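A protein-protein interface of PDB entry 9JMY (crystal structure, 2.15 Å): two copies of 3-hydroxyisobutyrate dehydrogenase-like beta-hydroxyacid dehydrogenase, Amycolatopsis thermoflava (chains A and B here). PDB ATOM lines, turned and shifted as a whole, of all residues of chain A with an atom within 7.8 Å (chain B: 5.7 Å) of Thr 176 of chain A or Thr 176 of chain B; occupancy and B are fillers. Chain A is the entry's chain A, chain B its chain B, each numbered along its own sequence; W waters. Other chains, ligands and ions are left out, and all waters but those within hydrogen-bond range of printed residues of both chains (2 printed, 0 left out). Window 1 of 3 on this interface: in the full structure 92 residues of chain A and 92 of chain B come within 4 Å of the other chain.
The side-chain hydroxyl (OG) of Ser 179 of chain B sits at hydrogen-bond distance from the side-chain amide oxygen (OE1) of Gln 262 of chain A (2.6 Å).
Of the printed residues of chain B, Val 173 of chain A touches Ala 180 (3.98 Å) and Tyr 181 (3.6 Å).
Thr 176 of chain A touches four residues of chain B.
Printed residues of chain B within 4 Å of Ser 177 of chain A: Ser 177 (3.8 Å).
Printed residues of chain B within 4 Å of Ile 242 of chain A: Leu 171 (3.6 Å) and Thr 172 (3.1 Å).
Lys 260 of chain A touches none of the printed residues of chain B.
Thr 176 of chain B touches four residues of chain A.
Of the printed residues of chain A, Tyr 181 of chain B touches Val 173 (3.6 Å) and Ala 209 (3.4 Å).
The nearest residue of chain B that does not touch Thr 176 of chain A is Ser 177 of chain B (5.6 Å).
The nearest residue of chain A that does not touch Thr 176 of chain B is Ser 177 of chain A (5.7 Å).
The backbone carbonyl oxygen of Val 173 of chain A is in hydrogen-bond range of the side-chain hydroxyl of Ser 177 of chain A (2.6 Å).
The backbone carbonyl oxygen (O) of Thr 172 of chain A sits at hydrogen-bond distance from the side-chain hydroxyl (OG1) of Thr 176 of chain A, 2.7 Å away.
The side-chain hydroxyl of Thr 176 of chain B is in hydrogen-bond range of the backbone carbonyl oxygen of Thr 172 of chain B, 2.7 Å away.
The backbone carbonyl oxygen (O) of Val 173 of chain B sits at hydrogen-bond distance from the side-chain hydroxyl (OG) of Ser 177 of chain B.
Thr 172 of chain A touches Ala 180 of chain B, and with the chains exchanged Ala 180 of chain A touches Thr 172 of chain B.
Val 173 of chain A touches Ala 180 of chain B, but with the chains exchanged Ala 180 of chain A does not touch Val 173 of chain B (4.1 Å).
Val 173 of chain A touches Tyr 181 of chain B, and with the chains exchanged Tyr 181 of chain A touches Val 173 of chain B.
Thr 176 of chain A touches Ala 180 of chain B, and with the chains exchanged Ala 180 of chain A touches Thr 176 of chain B.
Of the 25 pairs that touch across the chains among the printed residues, 13 have their exchanged pair printed and touching as well.
Of the 13 printed residues of chain B, 12 touch a printed residue of chain A.
Of the 24 printed residues of chain A, 14 touch a printed residue of chain B.
Printed residues of chain A that touch a printed residue of chain B: Thr 172, Val 173, Thr 176, Ser 177, Ala 180, Tyr 181, Gln 183, Ala 209, Ile 242, Leu 255, Ala 258, Val 259, Gln 262 and Tyr 263.
Hydrophobic or aromatic side chains of chain A that line the printed part of chain B: Val 173, Ala 180, Tyr 181, Ala 209, Ile 242, Leu 255, Ala 258, Val 259 and Tyr 263.
Among the printed residues, 25 pairs touch across the chains.
Among the printed residues, no Asp or Glu carboxylate lies within 4 Å of a Lys or Arg side-chain nitrogen of the other chain.
O of Thr 172 of chain A touches CB of Ala 180 of chain B, 3.8 Å away.
CG2 of Thr 176 of chain B touches CG2 of Thr 176 of chain A, 3.5 Å away.
Thr 176 of chain A touches Leu 255 of chain B (CG2 to CD2, 3.8 Å).
Val 259 of chain B touches Thr 176 of chain A.
CG2 of Thr 172 of chain B touches O of Ala 180 of chain A, 3.7 Å away.
Ile 242 of chain A touches Thr 172 of chain B (CG2 to OG1, 3.1 Å).
Ala 258 of chain A touches Leu 255 of chain B (CB to CA, 3.9 Å).
Val 259 of chain A touches Ser 179 of chain B.
CB of Leu 255 of chain B touches NE2 of Gln 262 of chain A (3.99 Å).
Tyr 263 of chain A touches Leu 175 of chain B.
Water W2 lies within hydrogen-bond range of the backbone carbonyl oxygen of Leu 175 of chain B, the side-chain hydroxyl of Tyr 263 of chain A and the side-chain hydroxyl of Ser 179 of chain B.
Water W1 bridges N of Leu 255 of chain B (2.9 Å) and NE2 of Gln 262 of chain A (3.0 Å).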
ATOM      1  N   ALA A 169     -20.554  35.706  21.761  1.00  0.00           N
ATOM      2  CA  ALA A 169     -19.485  35.798  20.731  1.00  0.00           C
ATOM      3  C   ALA A 169     -18.231  35.082  21.239  1.00  0.00           C
ATOM      4  O   ALA A 169     -17.589  34.351  20.468  1.00  0.00           O
ATOM      5  CB  ALA A 169     -19.189  37.239  20.400  1.00  0.00           C
ATOM      6  N   GLU A 170     -17.900  35.316  22.504  1.00  0.00           N
ATOM      7  CA  GLU A 170     -16.781  34.644  23.208  1.00  0.00           C
ATOM      8  C   GLU A 170     -16.995  33.129  23.193  1.00  0.00           C
ATOM      9  O   GLU A 170     -16.026  32.403  22.916  1.00  0.00           O
ATOM     10  CB  GLU A 170     -16.670  35.175  24.631  1.00  0.00           C
ATOM     11  CG  GLU A 170     -16.115  36.578  24.687  1.00  0.00           C
ATOM     12  CD  GLU A 170     -14.630  36.616  24.396  1.00  0.00           C
ATOM     13  OE1 GLU A 170     -13.841  36.364  25.344  1.00  0.00           O
ATOM     14  OE2 GLU A 170     -14.266  36.832  23.217  1.00  0.00           O
ATOM     15  N   LEU A 171     -18.216  32.649  23.469  1.00  0.00           N
ATOM     16  CA  LEU A 171     -18.452  31.185  23.572  1.00  0.00           C
ATOM     17  C   LEU A 171     -18.566  30.601  22.166  1.00  0.00           C
ATOM     18  O   LEU A 171     -18.381  29.400  22.017  1.00  0.00           O
ATOM     19  CB  LEU A 171     -19.679  30.892  24.431  1.00  0.00           C
ATOM     20  CG  LEU A 171     -19.413  30.713  25.931  1.00  0.00           C
ATOM     21  CD1 LEU A 171     -18.710  29.397  26.199  1.00  0.00           C
ATOM     22  CD2 LEU A 171     -18.624  31.885  26.507  1.00  0.00           C
ATOM     23  N   THR A 172     -18.853  31.418  21.152  1.00  0.00           N
ATOM     24  CA  THR A 172     -18.721  30.953  19.758  1.00  0.00           C
ATOM     25  C   THR A 172     -17.256  30.546  19.556  1.00  0.00           C
ATOM     26  O   THR A 172     -17.016  29.481  18.982  1.00  0.00           O
ATOM     27  CB  THR A 172     -19.155  32.018  18.746  1.00  0.00           C
ATOM     28  OG1 THR A 172     -20.496  32.432  19.012  1.00  0.00           O
ATOM     29  CG2 THR A 172     -19.029  31.490  17.335  1.00  0.00           C
ATOM     30  N   VAL A 173     -16.311  31.370  20.008  1.00  0.00           N
ATOM     31  CA  VAL A 173     -14.857  31.055  19.842  1.00  0.00           C
ATOM     32  C   VAL A 173     -14.542  29.818  20.691  1.00  0.00           C
ATOM     33  O   VAL A 173     -13.930  28.845  20.162  1.00  0.00           O
ATOM     34  CB  VAL A 173     -13.967  32.261  20.173  1.00  0.00           C
ATOM     35  CG1 VAL A 173     -12.476  31.918  20.106  1.00  0.00           C
ATOM     36  CG2 VAL A 173     -14.269  33.416  19.236  1.00  0.00           C
ATOM     37  N   PHE A 174     -14.991  29.830  21.947  1.00  0.00           N
ATOM     38  CA  PHE A 174     -14.590  28.818  22.962  1.00  0.00           C
ATOM     39  C   PHE A 174     -15.137  27.438  22.595  1.00  0.00           C
ATOM     40  O   PHE A 174     -14.320  26.521  22.430  1.00  0.00           O
ATOM     41  CB  PHE A 174     -15.024  29.262  24.356  1.00  0.00           C
ATOM     42  CG  PHE A 174     -14.584  28.330  25.442  1.00  0.00           C
ATOM     43  CD1 PHE A 174     -13.271  28.319  25.881  1.00  0.00           C
ATOM     44  CD2 PHE A 174     -15.467  27.408  25.966  1.00  0.00           C
ATOM     45  CE1 PHE A 174     -12.870  27.437  26.870  1.00  0.00           C
ATOM     46  CE2 PHE A 174     -15.063  26.523  26.948  1.00  0.00           C
ATOM     47  CZ  PHE A 174     -13.768  26.549  27.407  1.00  0.00           C
ATOM     48  N   LEU A 175     -16.459  27.288  22.463  1.00  0.00           N
ATOM     49  CA  LEU A 175     -17.111  25.968  22.185  1.00  0.00           C
ATOM     50  C   LEU A 175     -16.662  25.437  20.823  1.00  0.00           C
ATOM     51  O   LEU A 175     -16.343  24.223  20.718  1.00  0.00           O
ATOM     52  CB  LEU A 175     -18.639  26.110  22.246  1.00  0.00           C
ATOM     53  CG  LEU A 175     -19.179  26.459  23.636  1.00  0.00           C
ATOM     54  CD1 LEU A 175     -20.683  26.545  23.619  1.00  0.00           C
ATOM     55  CD2 LEU A 175     -18.677  25.443  24.667  1.00  0.00           C
ATOM     56  N   THR A 176     -16.608  26.298  19.804  1.00  0.00           N
ATOM     57  CA  THR A 176     -16.159  25.849  18.463  1.00  0.00           C
ATOM     58  C   THR A 176     -14.695  25.372  18.551  1.00  0.00           C
ATOM     59  O   THR A 176     -14.383  24.381  17.878  1.00  0.00           O
ATOM     60  CB  THR A 176     -16.388  26.904  17.373  1.00  0.00           C
ATOM     61  OG1 THR A 176     -17.728  27.392  17.448  1.00  0.00           O
ATOM     62  CG2 THR A 176     -16.162  26.335  15.986  1.00  0.00           C
ATOM     63  N   SER A 177     -13.835  26.021  19.347  1.00  0.00           N
ATOM     64  CA  SER A 177     -12.419  25.601  19.487  1.00  0.00           C
ATOM     65  C   SER A 177     -12.356  24.219  20.147  1.00  0.00           C
ATOM     66  O   SER A 177     -11.634  23.334  19.618  1.00  0.00           O
ATOM     67  CB  SER A 177     -11.570  26.629  20.192  1.00  0.00           C
ATOM     68  OG  SER A 177     -11.589  27.858  19.463  1.00  0.00           O
ATOM     69  N   LEU A 178     -13.107  24.027  21.228  1.00  0.00           N
ATOM     70  CA  LEU A 178     -13.168  22.726  21.936  1.00  0.00           C
ATOM     71  C   LEU A 178     -13.606  21.647  20.956  1.00  0.00           C
ATOM     72  O   LEU A 178     -12.937  20.622  20.890  1.00  0.00           O
ATOM     73  CB  LEU A 178     -14.133  22.822  23.116  1.00  0.00           C
ATOM     74  CG  LEU A 178     -13.705  23.738  24.262  1.00  0.00           C
ATOM     75  CD1 LEU A 178     -14.498  23.417  25.512  1.00  0.00           C
ATOM     76  CD2 LEU A 178     -12.220  23.633  24.562  1.00  0.00           C
ATOM     77  N   SER A 179     -14.658  21.888  20.169  1.00  0.00           N
ATOM     78  CA  SER A 179     -15.140  20.897  19.177  1.00  0.00           C
ATOM     79  C   SER A 179     -14.077  20.646  18.104  1.00  0.00           C
ATOM     80  O   SER A 179     -13.956  19.483  17.671  1.00  0.00           O
ATOM     81  CB  SER A 179     -16.470  21.267  18.607  1.00  0.00           C
ATOM     82  OG  SER A 179     -17.486  20.927  19.542  1.00  0.00           O
ATOM     83  N   ALA A 180     -13.289  21.657  17.711  1.00  0.00           N
ATOM     84  CA  ALA A 180     -12.232  21.483  16.684  1.00  0.00           C
ATOM     85  C   ALA A 180     -11.130  20.584  17.265  1.00  0.00           C
ATOM     86  O   ALA A 180     -10.559  19.744  16.526  1.00  0.00           O
ATOM     87  CB  ALA A 180     -11.715  22.826  16.229  1.00  0.00           C
ATOM     88  N   TYR A 181     -10.879  20.711  18.568  1.00  0.00           N
ATOM     89  CA  TYR A 181      -9.935  19.844  19.314  1.00  0.00           C
ATOM     90  C   TYR A 181     -10.423  18.394  19.289  1.00  0.00           C
ATOM     91  O   TYR A 181      -9.619  17.509  18.959  1.00  0.00           O
ATOM     92  CB  TYR A 181      -9.743  20.324  20.751  1.00  0.00           C
ATOM     93  CG  TYR A 181      -9.085  21.668  20.934  1.00  0.00           C
ATOM     94  CD1 TYR A 181      -8.259  22.235  19.982  1.00  0.00           C
ATOM     95  CD2 TYR A 181      -9.246  22.350  22.124  1.00  0.00           C
ATOM     96  CE1 TYR A 181      -7.625  23.443  20.212  1.00  0.00           C
ATOM     97  CE2 TYR A 181      -8.629  23.562  22.361  1.00  0.00           C
ATOM     98  CZ  TYR A 181      -7.826  24.120  21.401  1.00  0.00           C
ATOM     99  OH  TYR A 181      -7.242  25.330  21.650  1.00  0.00           O
ATOM    100  N   LEU A 182     -11.683  18.139  19.635  1.00  0.00           N
ATOM    101  CA  LEU A 182     -12.260  16.771  19.553  1.00  0.00           C
ATOM    102  C   LEU A 182     -12.083  16.253  18.126  1.00  0.00           C
ATOM    103  O   LEU A 182     -11.710  15.065  17.931  1.00  0.00           O
ATOM    104  CB  LEU A 182     -13.752  16.825  19.876  1.00  0.00           C
ATOM    105  CG  LEU A 182     -14.135  17.055  21.326  1.00  0.00           C
ATOM    106  CD1 LEU A 182     -15.640  16.958  21.456  1.00  0.00           C
ATOM    107  CD2 LEU A 182     -13.446  16.048  22.232  1.00  0.00           C
ATOM    108  N   GLN A 183     -12.392  17.108  17.154  1.00  0.00           N
ATOM    109  CA  GLN A 183     -12.358  16.737  15.719  1.00  0.00           C
ATOM    110  C   GLN A 183     -10.936  16.319  15.350  1.00  0.00           C
ATOM    111  O   GLN A 183     -10.775  15.274  14.696  1.00  0.00           O
ATOM    112  CB  GLN A 183     -12.838  17.888  14.840  1.00  0.00           C
ATOM    113  CG  GLN A 183     -13.217  17.421  13.448  1.00  0.00           C
ATOM    114  CD  GLN A 183     -14.529  16.681  13.443  1.00  0.00           C
ATOM    115  OE1 GLN A 183     -15.475  17.067  14.129  1.00  0.00           O
ATOM    116  NE2 GLN A 183     -14.612  15.642  12.624  1.00  0.00           N
ATOM    117  N   ALA A 209      -3.440  30.999  15.251  1.00  0.00           N
ATOM    118  CA  ALA A 209      -4.806  31.451  14.907  1.00  0.00           C
ATOM    119  C   ALA A 209      -5.098  32.800  15.587  1.00  0.00           C
ATOM    120  O   ALA A 209      -5.496  33.748  14.868  1.00  0.00           O
ATOM    121  CB  ALA A 209      -5.820  30.390  15.261  1.00  0.00           C
ATOM    122  N   ILE A 242      -9.761  17.856   5.088  1.00  0.00           N
ATOM    123  CA  ILE A 242     -10.130  17.501   6.494  1.00  0.00           C
ATOM    124  C   ILE A 242     -11.430  16.701   6.421  1.00  0.00           C
ATOM    125  O   ILE A 242     -11.540  15.646   7.075  1.00  0.00           O
ATOM    126  CB  ILE A 242     -10.270  18.764   7.376  1.00  0.00           C
ATOM    127  CG1 ILE A 242      -8.916  19.425   7.612  1.00  0.00           C
ATOM    128  CG2 ILE A 242     -10.958  18.464   8.702  1.00  0.00           C
ATOM    129  CD1 ILE A 242      -9.011  20.838   8.122  1.00  0.00           C
ATOM    130  N   LEU A 255     -18.719  19.181  11.787  1.00  0.00           N
ATOM    131  CA  LEU A 255     -17.910  20.413  12.023  1.00  0.00           C
ATOM    132  C   LEU A 255     -17.039  20.728  10.801  1.00  0.00           C
ATOM    133  O   LEU A 255     -17.099  21.845  10.285  1.00  0.00           O
ATOM    134  CB  LEU A 255     -17.097  20.289  13.319  1.00  0.00           C
ATOM    135  CG  LEU A 255     -16.317  21.529  13.745  1.00  0.00           C
ATOM    136  CD1 LEU A 255     -17.247  22.652  14.131  1.00  0.00           C
ATOM    137  CD2 LEU A 255     -15.371  21.226  14.897  1.00  0.00           C
ATOM    138  N   PRO A 256     -16.273  19.767  10.241  1.00  0.00           N
ATOM    139  CA  PRO A 256     -15.548  19.994   8.990  1.00  0.00           C
ATOM    140  C   PRO A 256     -16.452  20.416   7.824  1.00  0.00           C
ATOM    141  O   PRO A 256     -16.046  21.241   7.024  1.00  0.00           O
ATOM    142  CB  PRO A 256     -14.891  18.653   8.627  1.00  0.00           C
ATOM    143  CG  PRO A 256     -14.999  17.797   9.887  1.00  0.00           C
ATOM    144  CD  PRO A 256     -16.060  18.414  10.779  1.00  0.00           C
ATOM    145  N   ALA A 258     -19.353  22.148   8.096  1.00  0.00           N
ATOM    146  CA  ALA A 258     -19.744  23.569   8.295  1.00  0.00           C
ATOM    147  C   ALA A 258     -18.631  24.513   7.772  1.00  0.00           C
ATOM    148  O   ALA A 258     -18.934  25.494   7.057  1.00  0.00           O
ATOM    149  CB  ALA A 258     -20.056  23.838   9.731  1.00  0.00           C
ATOM    150  N   VAL A 259     -17.378  24.223   8.118  1.00  0.00           N
ATOM    151  CA  VAL A 259     -16.199  25.073   7.774  1.00  0.00           C
ATOM    152  C   VAL A 259     -16.011  25.015   6.261  1.00  0.00           C
ATOM    153  O   VAL A 259     -15.894  26.076   5.649  1.00  0.00           O
ATOM    154  CB  VAL A 259     -14.927  24.630   8.519  1.00  0.00           C
ATOM    155  CG1 VAL A 259     -13.733  25.444   8.085  1.00  0.00           C
ATOM    156  CG2 VAL A 259     -15.068  24.746  10.025  1.00  0.00           C
ATOM    157  N   LYS A 260     -16.047  23.818   5.674  1.00  0.00           N
ATOM    158  CA  LYS A 260     -15.907  23.668   4.209  1.00  0.00           C
ATOM    159  C   LYS A 260     -17.020  24.440   3.481  1.00  0.00           C
ATOM    160  O   LYS A 260     -16.706  25.048   2.427  1.00  0.00           O
ATOM    161  CB  LYS A 260     -15.859  22.194   3.815  1.00  0.00           C
ATOM    162  CG  LYS A 260     -15.801  21.930   2.317  1.00  0.00           C
ATOM    163  CD  LYS A 260     -16.788  20.873   1.907  1.00  0.00           C
ATOM    164  CE  LYS A 260     -16.862  20.616   0.412  1.00  0.00           C
ATOM    165  NZ  LYS A 260     -18.140  21.072  -0.160  1.00  0.00           N
ATOM    166  N   GLN A 262     -18.372  27.228   4.218  1.00  0.00           N
ATOM    167  CA  GLN A 262     -17.981  28.661   4.186  1.00  0.00           C
ATOM    168  C   GLN A 262     -17.049  28.895   2.981  1.00  0.00           C
ATOM    169  O   GLN A 262     -17.259  29.863   2.264  1.00  0.00           O
ATOM    170  CB  GLN A 262     -17.339  29.075   5.511  1.00  0.00           C
ATOM    171  CG  GLN A 262     -18.253  28.874   6.717  1.00  0.00           C
ATOM    172  CD  GLN A 262     -17.721  29.522   7.971  1.00  0.00           C
ATOM    173  OE1 GLN A 262     -16.562  29.929   8.031  1.00  0.00           O
ATOM    174  NE2 GLN A 262     -18.556  29.590   9.004  1.00  0.00           N
ATOM    175  N   TYR A 263     -16.043  28.044   2.779  1.00  0.00           N
ATOM    176  CA  TYR A 263     -15.085  28.143   1.653  1.00  0.00           C
ATOM    177  C   TYR A 263     -15.842  27.904   0.341  1.00  0.00           C
ATOM    178  O   TYR A 263     -15.766  28.763  -0.553  1.00  0.00           O
ATOM    179  CB  TYR A 263     -13.869  27.234   1.860  1.00  0.00           C
ATOM    180  CG  TYR A 263     -12.931  27.764   2.903  1.00  0.00           C
ATOM    181  CD1 TYR A 263     -11.910  28.643   2.574  1.00  0.00           C
ATOM    182  CD2 TYR A 263     -13.093  27.421   4.235  1.00  0.00           C
ATOM    183  CE1 TYR A 263     -11.066  29.154   3.544  1.00  0.00           C
ATOM    184  CE2 TYR A 263     -12.242  27.908   5.209  1.00  0.00           C
ATOM    185  CZ  TYR A 263     -11.235  28.792   4.875  1.00  0.00           C
ATOM    186  OH  TYR A 263     -10.436  29.294   5.873  1.00  0.00           O
ATOM    187  N   LEU B 171      -4.794  21.580  10.981  1.00  0.00           N
ATOM    188  CA  LEU B 171      -5.558  22.552  10.167  1.00  0.00           C
ATOM    189  C   LEU B 171      -7.046  22.530  10.565  1.00  0.00           C
ATOM    190  O   LEU B 171      -7.667  23.576  10.442  1.00  0.00           O
ATOM    191  CB  LEU B 171      -5.316  22.285   8.680  1.00  0.00           C
ATOM    192  CG  LEU B 171      -4.173  23.109   8.072  1.00  0.00           C
ATOM    193  CD1 LEU B 171      -4.573  24.559   7.904  1.00  0.00           C
ATOM    194  CD2 LEU B 171      -2.900  23.064   8.906  1.00  0.00           C
ATOM    195  N   THR B 172      -7.581  21.394  11.032  1.00  0.00           N
ATOM    196  CA  THR B 172      -8.923  21.281  11.650  1.00  0.00           C
ATOM    197  C   THR B 172      -8.963  22.303  12.780  1.00  0.00           C
ATOM    198  O   THR B 172      -9.920  23.104  12.827  1.00  0.00           O
ATOM    199  CB  THR B 172      -9.226  19.874  12.209  1.00  0.00           C
ATOM    200  OG1 THR B 172      -9.159  18.900  11.173  1.00  0.00           O
ATOM    201  CG2 THR B 172     -10.597  19.756  12.824  1.00  0.00           C
ATOM    202  N   VAL B 173      -7.924  22.340  13.618  1.00  0.00           N
ATOM    203  CA  VAL B 173      -7.938  23.290  14.762  1.00  0.00           C
ATOM    204  C   VAL B 173      -7.868  24.721  14.194  1.00  0.00           C
ATOM    205  O   VAL B 173      -8.630  25.601  14.638  1.00  0.00           O
ATOM    206  CB  VAL B 173      -6.825  22.987  15.781  1.00  0.00           C
ATOM    207  CG1 VAL B 173      -6.779  24.044  16.874  1.00  0.00           C
ATOM    208  CG2 VAL B 173      -6.942  21.605  16.387  1.00  0.00           C
ATOM    209  N   PHE B 174      -6.954  24.946  13.255  1.00  0.00           N
ATOM    210  CA  PHE B 174      -6.559  26.298  12.802  1.00  0.00           C
ATOM    211  C   PHE B 174      -7.720  26.913  12.025  1.00  0.00           C
ATOM    212  O   PHE B 174      -8.160  28.011  12.407  1.00  0.00           O
ATOM    213  CB  PHE B 174      -5.278  26.249  11.982  1.00  0.00           C
ATOM    214  CG  PHE B 174      -4.850  27.610  11.486  1.00  0.00           C
ATOM    215  CD1 PHE B 174      -4.306  28.550  12.349  1.00  0.00           C
ATOM    216  CD2 PHE B 174      -5.077  27.984  10.180  1.00  0.00           C
ATOM    217  CE1 PHE B 174      -3.922  29.802  11.890  1.00  0.00           C
ATOM    218  CE2 PHE B 174      -4.681  29.235   9.716  1.00  0.00           C
ATOM    219  CZ  PHE B 174      -4.084  30.130  10.566  1.00  0.00           C
ATOM    220  N   LEU B 175      -8.205  26.218  10.994  1.00  0.00           N
ATOM    221  CA  LEU B 175      -9.257  26.749  10.096  1.00  0.00           C
ATOM    222  C   LEU B 175     -10.572  26.933  10.870  1.00  0.00           C
ATOM    223  O   LEU B 175     -11.287  27.955  10.625  1.00  0.00           O
ATOM    224  CB  LEU B 175      -9.450  25.792   8.914  1.00  0.00           C
ATOM    225  CG  LEU B 175      -8.302  25.747   7.911  1.00  0.00           C
ATOM    226  CD1 LEU B 175      -8.624  24.745   6.797  1.00  0.00           C
ATOM    227  CD2 LEU B 175      -8.020  27.132   7.330  1.00  0.00           C
ATOM    228  N   THR B 176     -10.925  25.986  11.745  1.00  0.00           N
ATOM    229  CA  THR B 176     -12.225  26.054  12.454  1.00  0.00           C
ATOM    230  C   THR B 176     -12.157  27.236  13.433  1.00  0.00           C
ATOM    231  O   THR B 176     -13.167  27.948  13.594  1.00  0.00           O
ATOM    232  CB  THR B 176     -12.572  24.747  13.176  1.00  0.00           C
ATOM    233  OG1 THR B 176     -12.479  23.662  12.257  1.00  0.00           O
ATOM    234  CG2 THR B 176     -13.938  24.826  13.812  1.00  0.00           C
ATOM    235  N   SER B 177     -10.990  27.462  14.024  1.00  0.00           N
ATOM    236  CA  SER B 177     -10.756  28.630  14.912  1.00  0.00           C
ATOM    237  C   SER B 177     -10.978  29.922  14.110  1.00  0.00           C
ATOM    238  O   SER B 177     -11.715  30.782  14.603  1.00  0.00           O
ATOM    239  CB  SER B 177      -9.393  28.589  15.557  1.00  0.00           C
ATOM    240  OG  SER B 177      -9.262  27.471  16.440  1.00  0.00           O
ATOM    241  N   LEU B 178     -10.397  30.034  12.907  1.00  0.00           N
ATOM    242  CA  LEU B 178     -10.558  31.238  12.042  1.00  0.00           C
ATOM    243  C   LEU B 178     -12.036  31.452  11.704  1.00  0.00           C
ATOM    244  O   LEU B 178     -12.471  32.582  11.795  1.00  0.00           O
ATOM    245  CB  LEU B 178      -9.732  31.114  10.763  1.00  0.00           C
ATOM    246  CG  LEU B 178      -8.212  31.127  10.920  1.00  0.00           C
ATOM    247  CD1 LEU B 178      -7.587  31.202   9.547  1.00  0.00           C
ATOM    248  CD2 LEU B 178      -7.728  32.284  11.776  1.00  0.00           C
ATOM    249  N   SER B 179     -12.773  30.392  11.359  1.00  0.00           N
ATOM    250  CA  SER B 179     -14.238  30.432  11.127  1.00  0.00           C
ATOM    251  C   SER B 179     -14.984  30.810  12.416  1.00  0.00           C
ATOM    252  O   SER B 179     -15.966  31.535  12.315  1.00  0.00           O
ATOM    253  CB  SER B 179     -14.725  29.140  10.570  1.00  0.00           C
ATOM    254  OG  SER B 179     -14.382  29.019   9.212  1.00  0.00           O
ATOM    255  N   ALA B 180     -14.532  30.385  13.598  1.00  0.00           N
ATOM    256  CA  ALA B 180     -15.189  30.790  14.870  1.00  0.00           C
ATOM    257  C   ALA B 180     -14.991  32.296  15.103  1.00  0.00           C
ATOM    258  O   ALA B 180     -15.934  32.957  15.571  1.00  0.00           O
ATOM    259  CB  ALA B 180     -14.663  29.978  16.016  1.00  0.00           C
ATOM    260  N   TYR B 181     -13.819  32.836  14.774  1.00  0.00           N
ATOM    261  CA  TYR B 181     -13.556  34.291  14.872  1.00  0.00           C
ATOM    262  C   TYR B 181     -14.515  35.059  13.941  1.00  0.00           C
ATOM    263  O   TYR B 181     -15.184  36.007  14.443  1.00  0.00           O
ATOM    264  CB  TYR B 181     -12.102  34.616  14.535  1.00  0.00           C
ATOM    265  CG  TYR B 181     -11.039  34.074  15.456  1.00  0.00           C
ATOM    266  CD1 TYR B 181     -11.292  33.785  16.788  1.00  0.00           C
ATOM    267  CD2 TYR B 181      -9.734  33.934  15.001  1.00  0.00           C
ATOM    268  CE1 TYR B 181     -10.287  33.317  17.622  1.00  0.00           C
ATOM    269  CE2 TYR B 181      -8.718  33.493  15.832  1.00  0.00           C
ATOM    270  CZ  TYR B 181      -9.001  33.166  17.140  1.00  0.00           C
ATOM    271  OH  TYR B 181      -8.001  32.740  17.966  1.00  0.00           O
ATOM    272  N   LEU B 255     -21.816  26.989  11.178  1.00  0.00           N
ATOM    273  CA  LEU B 255     -20.835  26.649  12.244  1.00  0.00           C
ATOM    274  C   LEU B 255     -21.551  26.412  13.578  1.00  0.00           C
ATOM    275  O   LEU B 255     -21.426  25.325  14.157  1.00  0.00           O
ATOM    276  CB  LEU B 255     -19.746  27.721  12.319  1.00  0.00           C
ATOM    277  CG  LEU B 255     -18.488  27.336  13.092  1.00  0.00           C
ATOM    278  CD1 LEU B 255     -17.781  26.138  12.481  1.00  0.00           C
ATOM    279  CD2 LEU B 255     -17.535  28.505  13.162  1.00  0.00           C
ATOM    280  N   VAL B 259     -21.865  22.806  15.780  1.00  0.00           N
ATOM    281  CA  VAL B 259     -21.440  22.680  17.211  1.00  0.00           C
ATOM    282  C   VAL B 259     -22.652  22.219  18.048  1.00  0.00           C
ATOM    283  O   VAL B 259     -22.514  21.218  18.778  1.00  0.00           O
ATOM    284  CB  VAL B 259     -20.806  23.973  17.756  1.00  0.00           C
ATOM    285  CG1 VAL B 259     -20.573  23.884  19.266  1.00  0.00           C
ATOM    286  CG2 VAL B 259     -19.505  24.274  17.038  1.00  0.00           C
HETATM  287  O   HOH W   1     -21.394  29.615   9.997  1.00  0.00           O
HETATM  288  O   HOH W   2     -11.652  29.076   8.262  1.00  0.00           O
